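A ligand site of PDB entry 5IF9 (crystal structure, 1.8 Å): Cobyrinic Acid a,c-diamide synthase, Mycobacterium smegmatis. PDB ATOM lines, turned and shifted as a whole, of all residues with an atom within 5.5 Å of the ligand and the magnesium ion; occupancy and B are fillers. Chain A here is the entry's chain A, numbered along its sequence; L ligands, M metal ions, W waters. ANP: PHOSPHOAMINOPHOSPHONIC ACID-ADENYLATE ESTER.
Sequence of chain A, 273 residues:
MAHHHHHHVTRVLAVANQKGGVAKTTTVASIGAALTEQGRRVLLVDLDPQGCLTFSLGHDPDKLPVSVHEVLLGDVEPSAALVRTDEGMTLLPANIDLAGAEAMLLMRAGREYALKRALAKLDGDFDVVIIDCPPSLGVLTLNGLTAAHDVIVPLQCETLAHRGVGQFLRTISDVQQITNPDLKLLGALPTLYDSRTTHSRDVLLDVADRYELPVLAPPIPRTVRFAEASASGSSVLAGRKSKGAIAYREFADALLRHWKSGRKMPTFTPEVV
An oxygen (O1A) of the ligand is in hydrogen-bond range of the backbone NH (N) of Thr 25 (3.4 Å).
N of Lys 24 lies within hydrogen-bond range of O1B of the ligand, 3.0 Å away.
An oxygen (O1G) of the ligand lies within salt-bridge range of the side-chain amino group of Lys 24.
N of Thr 26 is in hydrogen-bond range of O1A of the ligand (2.9 Å).
O1A of the ligand is in hydrogen-bond range of OG1 of Thr 26, 2.8 Å away.
A nitrogen (N1) of the ligand lies within hydrogen-bond range of the backbone NH (N) of Thr 223 (2.8 Å).
A nitrogen (N1) of the ligand sits at hydrogen-bond distance from the side-chain hydroxyl (OG1) of Thr 223 (3.3 Å).
The backbone NH (N) of Ala 23 is in hydrogen-bond range of an oxygen (O3A) of the ligand (2.9 Å).
The backbone carbonyl oxygen (O) of Pro 221 sits at hydrogen-bond distance from a nitrogen (N6) of the ligand (2.9 Å).
N of Val 22 sits at hydrogen-bond distance from O1B of the ligand.
The backbone NH (N) of Gly 21 is in hydrogen-bond range of an oxygen (O1G) of the ligand (3.2 Å).
The side-chain hydroxyl (OG1) of Thr 25 sits close to the side-chain carboxylate (OD1) of Asp 132.
The backbone carbonyl oxygen (O) of Lys 19 lies within hydrogen-bond range of the side-chain amino group (NZ) of Lys 24 (3.0 Å).
O of Asn 17 lies within hydrogen-bond range of NZ of Lys 24, at 3.0 Å.
The backbone NH (N) of Val 236 sits at hydrogen-bond distance from the side-chain hydroxyl (OG1) of Thr 26 (3.1 Å).
The backbone carbonyl oxygen (O) of Ala 23 lies within hydrogen-bond range of the side-chain hydroxyl (OG1) of Thr 27 (2.6 Å).
The backbone carbonyl oxygen of Cys 52 lies within hydrogen-bond range of the side-chain hydroxyl of Ser 235, 3.4 Å away.
The backbone NH (N) of Leu 192 sits at hydrogen-bond distance from the backbone carbonyl oxygen (O) of Ile 220 (3.2 Å).
The side-chain amide oxygen (OD1) of Asn 17 lies within hydrogen-bond range of the backbone NH (N) of Lys 19, at 2.9 Å.
Merely in contact with the ligand: Gly 20 (3.2 Å), Pro 135 (3.3 Å), Ser 235 (3.5 Å), Arg 222 (3.5 Å), Asp 48 (3.6 Å), Leu 192 (3.8 Å), Val 236 (3.9 Å) and Lys 19 (3.95 Å).
Hydrophobic or aromatic side chains within 4 Å of the ligand: Val 22, Ala 23, Pro 135, Leu 192 and Val 236.
The nearest printed residue that does not touch the ligand is Ile 220 (4.2 Å).
One residue has an atom within 4 Å of the magnesium ion: Thr 25.
The nearest printed residue that does not touch the magnesium ion is Asp 132 (4.1 Å).
The magnesium ion is bound by an oxygen (O3G) of the ligand, an oxygen (O2B) of the ligand, water W5, water W1, water W9 and the side-chain hydroxyl of Thr 25.
The magnesium ion has six donor atoms within binding distance.
Water W5 lies within hydrogen-bond range of O2A of the ligand (2.7 Å) and SG of Cys 52 (3.3 Å).
Water W1 bridges OD2 of Asp 48 and SG of Cys 52.
Water W6 bridges an oxygen (O2G) of the ligand (2.7 Å) and the side-chain carboxylate (OD2) of Asp 48 (2.8 Å).
Water W8 lies within hydrogen-bond range of a nitrogen (N6) of the ligand, the backbone NH of Leu 192, the backbone carbonyl oxygen of Ile 220 and the backbone carbonyl oxygen of Pro 221.
Water W2 lies within hydrogen-bond range of a nitrogen (N7) of the ligand (2.7 Å) and the side-chain hydroxyl of Tyr 248 (2.8 Å).
Water W4 bridges O4' of the ligand (3.0 Å) and NH2 of Arg 222 (3.4 Å).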
ATOM      1  N   ASN A  17       0.991  10.307  16.343  1.00  0.00           N
ATOM      2  CA  ASN A  17       1.673  11.455  15.742  1.00  0.00           C
ATOM      3  C   ASN A  17       2.225  10.933  14.412  1.00  0.00           C
ATOM      4  O   ASN A  17       2.988   9.963  14.416  1.00  0.00           O
ATOM      5  CB  ASN A  17       2.795  11.991  16.637  1.00  0.00           C
ATOM      6  CG  ASN A  17       3.430  13.277  16.082  1.00  0.00           C
ATOM      7  OD1 ASN A  17       3.281  13.598  14.900  1.00  0.00           O
ATOM      8  ND2 ASN A  17       4.141  14.023  16.949  1.00  0.00           N
ATOM      9  N   LYS A  19       4.353  12.223  12.539  1.00  0.00           N
ATOM     10  CA  LYS A  19       5.786  12.470  12.442  1.00  0.00           C
ATOM     11  C   LYS A  19       6.548  11.304  13.054  1.00  0.00           C
ATOM     12  O   LYS A  19       6.242  10.846  14.159  1.00  0.00           O
ATOM     13  CB  LYS A  19       6.130  13.778  13.169  1.00  0.00           C
ATOM     14  CG  LYS A  19       7.565  14.282  12.981  1.00  0.00           C
ATOM     15  CD  LYS A  19       7.894  14.567  11.521  1.00  0.00           C
ATOM     16  CE  LYS A  19       9.289  15.169  11.384  1.00  0.00           C
ATOM     17  NZ  LYS A  19       9.443  16.418  12.181  1.00  0.00           N
ATOM     18  N   GLY A  20       7.555  10.808  12.331  1.00  0.00           N
ATOM     19  CA  GLY A  20       8.285   9.640  12.782  1.00  0.00           C
ATOM     20  C   GLY A  20       9.353   9.984  13.807  1.00  0.00           C
ATOM     21  O   GLY A  20       9.976  11.046  13.774  1.00  0.00           O
ATOM     22  N   GLY A  21       9.582   9.049  14.715  1.00  0.00           N
ATOM     23  CA  GLY A  21      10.759   9.138  15.563  1.00  0.00           C
ATOM     24  C   GLY A  21      10.593  10.053  16.755  1.00  0.00           C
ATOM     25  O   GLY A  21      11.590  10.549  17.270  1.00  0.00           O
ATOM     26  N   VAL A  22       9.363  10.248  17.226  1.00  0.00           N
ATOM     27  CA  VAL A  22       9.063  11.200  18.288  1.00  0.00           C
ATOM     28  C   VAL A  22       8.756  10.512  19.607  1.00  0.00           C
ATOM     29  O   VAL A  22       8.222  11.136  20.523  1.00  0.00           O
ATOM     30  CB  VAL A  22       7.916  12.143  17.890  1.00  0.00           C
ATOM     31  CG1 VAL A  22       8.315  12.954  16.655  1.00  0.00           C
ATOM     32  CG2 VAL A  22       6.621  11.361  17.623  1.00  0.00           C
ATOM     33  N   ALA A  23       9.080   9.217  19.713  1.00  0.00           N
ATOM     34  CA  ALA A  23       8.960   8.393  20.924  1.00  0.00           C
ATOM     35  C   ALA A  23       7.527   7.943  21.220  1.00  0.00           C
ATOM     36  O   ALA A  23       7.168   7.750  22.382  1.00  0.00           O
ATOM     37  CB  ALA A  23       9.550   9.125  22.140  1.00  0.00           C
ATOM     38  N   LYS A  24       6.723   7.725  20.183  1.00  0.00           N
ATOM     39  CA  LYS A  24       5.421   7.098  20.388  1.00  0.00           C
ATOM     40  C   LYS A  24       5.576   5.735  21.044  1.00  0.00           C
ATOM     41  O   LYS A  24       4.956   5.458  22.079  1.00  0.00           O
ATOM     42  CB  LYS A  24       4.660   6.955  19.061  1.00  0.00           C
ATOM     43  CG  LYS A  24       4.202   8.270  18.418  1.00  0.00           C
ATOM     44  CD  LYS A  24       3.381   8.033  17.152  1.00  0.00           C
ATOM     45  CE  LYS A  24       4.198   7.444  16.007  1.00  0.00           C
ATOM     46  NZ  LYS A  24       5.321   8.359  15.535  1.00  0.00           N
ATOM     47  N   THR A  25       6.393   4.866  20.457  1.00  0.00           N
ATOM     48  CA  THR A  25       6.474   3.475  20.908  1.00  0.00           C
ATOM     49  C   THR A  25       7.097   3.388  22.295  1.00  0.00           C
ATOM     50  O   THR A  25       6.621   2.625  23.149  1.00  0.00           O
ATOM     51  CB  THR A  25       7.273   2.640  19.901  1.00  0.00           C
ATOM     52  OG1 THR A  25       6.564   2.625  18.662  1.00  0.00           O
ATOM     53  CG2 THR A  25       7.455   1.213  20.418  1.00  0.00           C
ATOM     54  N   THR A  26       8.169   4.142  22.519  1.00  0.00           N
ATOM     55  CA  THR A  26       8.761   4.221  23.854  1.00  0.00           C
ATOM     56  C   THR A  26       7.745   4.701  24.876  1.00  0.00           C
ATOM     57  O   THR A  26       7.718   4.234  26.020  1.00  0.00           O
ATOM     58  CB  THR A  26       9.984   5.152  23.829  1.00  0.00           C
ATOM     59  OG1 THR A  26      10.921   4.708  22.840  1.00  0.00           O
ATOM     60  CG2 THR A  26      10.665   5.197  25.191  1.00  0.00           C
ATOM     61  N   THR A  27       6.894   5.642  24.467  1.00  0.00           N
ATOM     62  CA  THR A  27       5.880   6.178  25.370  1.00  0.00           C
ATOM     63  C   THR A  27       4.822   5.131  25.691  1.00  0.00           C
ATOM     64  O   THR A  27       4.447   4.970  26.853  1.00  0.00           O
ATOM     65  CB  THR A  27       5.250   7.434  24.757  1.00  0.00           C
ATOM     66  OG1 THR A  27       6.221   8.490  24.715  1.00  0.00           O
ATOM     67  CG2 THR A  27       4.041   7.872  25.544  1.00  0.00           C
ATOM     68  N   ASP A  48       1.713  -0.653  14.300  1.00  0.00           N
ATOM     69  CA  ASP A  48       2.735  -0.380  13.289  1.00  0.00           C
ATOM     70  C   ASP A  48       3.140  -1.678  12.620  1.00  0.00           C
ATOM     71  O   ASP A  48       3.653  -2.586  13.310  1.00  0.00           O
ATOM     72  CB  ASP A  48       3.949   0.299  13.940  1.00  0.00           C
ATOM     73  CG  ASP A  48       4.896   0.924  12.904  1.00  0.00           C
ATOM     74  OD1 ASP A  48       4.832   0.550  11.731  1.00  0.00           O
ATOM     75  OD2 ASP A  48       5.702   1.792  13.293  1.00  0.00           O
ATOM     76  N   CYS A  52       7.675  -2.234  15.959  1.00  0.00           N
ATOM     77  CA  CYS A  52       8.674  -1.748  16.897  1.00  0.00           C
ATOM     78  C   CYS A  52       8.309  -2.085  18.336  1.00  0.00           C
ATOM     79  O   CYS A  52       9.160  -2.514  19.117  1.00  0.00           O
ATOM     80  CB  CYS A  52       8.861  -0.238  16.737  1.00  0.00           C
ATOM     81  SG  CYS A  52       9.174   0.227  15.012  1.00  0.00           S
ATOM     82  N   ASP A 132      -0.464   1.879  20.122  1.00  0.00           N
ATOM     83  CA  ASP A 132       0.719   2.481  19.512  1.00  0.00           C
ATOM     84  C   ASP A 132       0.449   2.697  18.026  1.00  0.00           C
ATOM     85  O   ASP A 132       0.436   1.744  17.242  1.00  0.00           O
ATOM     86  CB  ASP A 132       1.935   1.580  19.714  1.00  0.00           C
ATOM     87  CG  ASP A 132       3.253   2.248  19.280  1.00  0.00           C
ATOM     88  OD1 ASP A 132       4.224   1.493  19.092  1.00  0.00           O
ATOM     89  OD2 ASP A 132       3.303   3.503  19.163  1.00  0.00           O
ATOM     90  N   CYS A 133       0.263   3.962  17.615  1.00  0.00           N
ATOM     91  CA  CYS A 133      -0.081   4.195  16.218  1.00  0.00           C
ATOM     92  C   CYS A 133       1.185   4.387  15.371  1.00  0.00           C
ATOM     93  O   CYS A 133       2.206   4.867  15.869  1.00  0.00           O
ATOM     94  CB  CYS A 133      -0.971   5.427  16.084  1.00  0.00           C
ATOM     95  SG  CYS A 133      -2.612   5.213  16.846  1.00  0.00           S
ATOM     96  N   PRO A 134       1.136   3.980  14.101  1.00  0.00           N
ATOM     97  CA  PRO A 134       2.283   4.156  13.224  1.00  0.00           C
ATOM     98  C   PRO A 134       2.432   5.616  12.817  1.00  0.00           C
ATOM     99  O   PRO A 134       1.504   6.420  13.013  1.00  0.00           O
ATOM    100  CB  PRO A 134       1.935   3.277  12.010  1.00  0.00           C
ATOM    101  CG  PRO A 134       0.440   3.360  11.940  1.00  0.00           C
ATOM    102  CD  PRO A 134       0.007   3.333  13.402  1.00  0.00           C
ATOM    103  N   PRO A 135       3.642   6.018  12.201  1.00  0.00           N
ATOM    104  CA  PRO A 135       3.858   7.393  11.720  1.00  0.00           C
ATOM    105  C   PRO A 135       3.098   7.602  10.405  1.00  0.00           C
ATOM    106  O   PRO A 135       3.672   7.623   9.303  1.00  0.00           O
ATOM    107  CB  PRO A 135       5.376   7.456  11.527  1.00  0.00           C
ATOM    108  CG  PRO A 135       5.765   6.046  11.187  1.00  0.00           C
ATOM    109  CD  PRO A 135       4.859   5.176  12.058  1.00  0.00           C
ATOM    110  N   LEU A 192      12.012  13.935  24.141  1.00  0.00           N
ATOM    111  CA  LEU A 192      13.374  14.289  23.748  1.00  0.00           C
ATOM    112  C   LEU A 192      13.745  15.689  24.254  1.00  0.00           C
ATOM    113  O   LEU A 192      14.499  16.428  23.604  1.00  0.00           O
ATOM    114  CB  LEU A 192      13.547  14.174  22.224  1.00  0.00           C
ATOM    115  CG  LEU A 192      13.097  12.816  21.686  1.00  0.00           C
ATOM    116  CD1 LEU A 192      13.139  12.755  20.157  1.00  0.00           C
ATOM    117  CD2 LEU A 192      13.949  11.718  22.275  1.00  0.00           C
ATOM    118  N   ILE A 220       9.359  14.465  28.915  1.00  0.00           N
ATOM    119  CA  ILE A 220      10.220  13.295  28.994  1.00  0.00           C
ATOM    120  C   ILE A 220      11.607  13.710  28.516  1.00  0.00           C
ATOM    121  O   ILE A 220      11.743  14.066  27.341  1.00  0.00           O
ATOM    122  CB  ILE A 220       9.703  12.107  28.169  1.00  0.00           C
ATOM    123  CG1 ILE A 220       8.206  11.906  28.400  1.00  0.00           C
ATOM    124  CG2 ILE A 220      10.498  10.863  28.535  1.00  0.00           C
ATOM    125  CD1 ILE A 220       7.822  11.692  29.878  1.00  0.00           C
ATOM    126  N   PRO A 221      12.626  13.681  29.367  1.00  0.00           N
ATOM    127  CA  PRO A 221      13.944  14.130  28.919  1.00  0.00           C
ATOM    128  C   PRO A 221      14.561  13.129  27.966  1.00  0.00           C
ATOM    129  O   PRO A 221      14.255  11.932  27.994  1.00  0.00           O
ATOM    130  CB  PRO A 221      14.741  14.232  30.218  1.00  0.00           C
ATOM    131  CG  PRO A 221      14.101  13.195  31.107  1.00  0.00           C
ATOM    132  CD  PRO A 221      12.631  13.292  30.788  1.00  0.00           C
ATOM    133  N   ARG A 222      15.420  13.631  27.082  1.00  0.00           N
ATOM    134  CA  ARG A 222      16.268  12.731  26.318  1.00  0.00           C
ATOM    135  C   ARG A 222      17.317  12.119  27.242  1.00  0.00           C
ATOM    136  O   ARG A 222      17.918  12.814  28.062  1.00  0.00           O
ATOM    137  CB  ARG A 222      16.941  13.481  25.166  1.00  0.00           C
ATOM    138  CG  ARG A 222      18.070  12.691  24.515  1.00  0.00           C
ATOM    139  CD  ARG A 222      18.759  13.467  23.395  1.00  0.00           C
ATOM    140  NE  ARG A 222      17.956  13.495  22.172  1.00  0.00           N
ATOM    141  CZ  ARG A 222      17.858  12.486  21.322  1.00  0.00           C
ATOM    142  NH1 ARG A 222      18.516  11.348  21.546  1.00  0.00           N
ATOM    143  NH2 ARG A 222      17.102  12.590  20.230  1.00  0.00           N
ATOM    144  N   THR A 223      17.511  10.809  27.128  1.00  0.00           N
ATOM    145  CA  THR A 223      18.485  10.113  27.967  1.00  0.00           C
ATOM    146  C   THR A 223      19.652   9.569  27.139  1.00  0.00           C
ATOM    147  O   THR A 223      20.015  10.140  26.112  1.00  0.00           O
ATOM    148  CB  THR A 223      17.843   8.936  28.731  1.00  0.00           C
ATOM    149  OG1 THR A 223      17.457   7.916  27.794  1.00  0.00           O
ATOM    150  CG2 THR A 223      16.612   9.412  29.498  1.00  0.00           C
ATOM    151  N   SER A 235      13.101   1.000  19.447  1.00  0.00           N
ATOM    152  CA  SER A 235      12.443   1.778  20.488  1.00  0.00           C
ATOM    153  C   SER A 235      12.863   1.320  21.876  1.00  0.00           C
ATOM    154  O   SER A 235      13.594   0.340  22.013  1.00  0.00           O
ATOM    155  CB  SER A 235      10.919   1.680  20.332  1.00  0.00           C
ATOM    156  OG  SER A 235      10.513   0.335  20.392  1.00  0.00           O
ATOM    157  N   VAL A 236      12.392   2.007  22.919  1.00  0.00           N
ATOM    158  CA  VAL A 236      12.904   1.831  24.276  1.00  0.00           C
ATOM    159  C   VAL A 236      11.764   1.562  25.253  1.00  0.00           C
ATOM    160  O   VAL A 236      10.576   1.649  24.919  1.00  0.00           O
ATOM    161  CB  VAL A 236      13.724   3.045  24.748  1.00  0.00           C
ATOM    162  N   TYR A 248       8.088   9.425  33.079  1.00  0.00           N
ATOM    163  CA  TYR A 248       6.984   8.590  32.611  1.00  0.00           C
ATOM    164  C   TYR A 248       6.097   8.149  33.764  1.00  0.00           C
ATOM    165  O   TYR A 248       4.873   8.086  33.621  1.00  0.00           O
ATOM    166  CB  TYR A 248       7.529   7.366  31.876  1.00  0.00           C
ATOM    167  CG  TYR A 248       7.776   7.612  30.389  1.00  0.00           C
ATOM    168  CD1 TYR A 248       6.782   8.107  29.562  1.00  0.00           C
ATOM    169  CD2 TYR A 248       9.021   7.346  29.838  1.00  0.00           C
ATOM    170  CE1 TYR A 248       7.019   8.332  28.212  1.00  0.00           C
ATOM    171  CE2 TYR A 248       9.269   7.563  28.496  1.00  0.00           C
ATOM    172  CZ  TYR A 248       8.272   8.062  27.692  1.00  0.00           C
ATOM    173  OH  TYR A 248       8.528   8.257  26.351  1.00  0.00           O
HETATM  174  PG  ANP L   1       7.875   5.735  14.629  1.00  0.00           P
HETATM  175  O1G ANP L   1       7.201   7.010  14.223  1.00  0.00           O
HETATM  176  O2G ANP L   1       8.723   5.145  13.450  1.00  0.00           O
HETATM  177  O3G ANP L   1       6.839   4.680  15.116  1.00  0.00           O
HETATM  178  PB  ANP L   1       8.345   6.447  17.342  1.00  0.00           P
HETATM  179  O1B ANP L   1       7.555   7.706  17.328  1.00  0.00           O
HETATM  180  O2B ANP L   1       7.525   5.253  17.905  1.00  0.00           O
HETATM  181  N3B ANP L   1       9.010   6.103  15.841  1.00  0.00           N
HETATM  182  PA  ANP L   1      10.404   5.547  19.061  1.00  0.00           P
HETATM  183  O1A ANP L   1       9.811   5.194  20.371  1.00  0.00           O
HETATM  184  O2A ANP L   1      10.694   4.353  18.155  1.00  0.00           O
HETATM  185  O3A ANP L   1       9.572   6.691  18.316  1.00  0.00           O
HETATM  186  O5' ANP L   1      11.761   6.335  19.380  1.00  0.00           O
HETATM  187  C5' ANP L   1      12.566   6.885  18.313  1.00  0.00           C
HETATM  188  C4' ANP L   1      14.003   6.734  18.751  1.00  0.00           C
HETATM  189  O4' ANP L   1      14.255   7.612  19.872  1.00  0.00           O
HETATM  190  C3' ANP L   1      14.390   5.323  19.201  1.00  0.00           C
HETATM  191  O3' ANP L   1      15.709   4.995  18.775  1.00  0.00           O
HETATM  192  C2' ANP L   1      14.292   5.421  20.733  1.00  0.00           C
HETATM  193  O2' ANP L   1      15.136   4.486  21.403  1.00  0.00           O
HETATM  194  C1' ANP L   1      14.757   6.854  20.960  1.00  0.00           C
HETATM  195  N9  ANP L   1      14.249   7.443  22.197  1.00  0.00           N
HETATM  196  C8  ANP L   1      12.944   7.491  22.615  1.00  0.00           C
HETATM  197  N7  ANP L   1      12.774   8.089  23.769  1.00  0.00           N
HETATM  198  C5  ANP L   1      14.063   8.462  24.134  1.00  0.00           C
HETATM  199  C6  ANP L   1      14.563   9.153  25.262  1.00  0.00           C
HETATM  200  N6  ANP L   1      13.803   9.594  26.272  1.00  0.00           N
HETATM  201  N1  ANP L   1      15.898   9.368  25.304  1.00  0.00           N
HETATM  202  C2  ANP L   1      16.662   8.948  24.299  1.00  0.00           C
HETATM  203  N3  ANP L   1      16.293   8.290  23.192  1.00  0.00           N
HETATM  204  C4  ANP L   1      14.979   8.088  23.173  1.00  0.00           C
HETATM  205 MG    MG M   1       6.833   3.670  16.794  1.00  0.00          MG
HETATM  206  O   HOH W   1       6.240   1.867  15.805  1.00  0.00           O
HETATM  207  O   HOH W   2      10.982   9.211  25.490  1.00  0.00           O
HETATM  208  O   HOH W   3       9.302   6.531  10.930  1.00  0.00           O
HETATM  209  O   HOH W   4      16.053   9.740  18.714  1.00  0.00           O
HETATM  210  O   HOH W   5       8.790   3.000  16.790  1.00  0.00           O
HETATM  211  O   HOH W   6       8.028   2.912  12.189  1.00  0.00           O
HETATM  212  O   HOH W   7      12.411   3.497  16.392  1.00  0.00           O
HETATM  213  O   HOH W   8      12.214  11.607  25.529  1.00  0.00           O
HETATM  214  O   HOH W   9       4.768   4.186  17.126  1.00  0.00           O
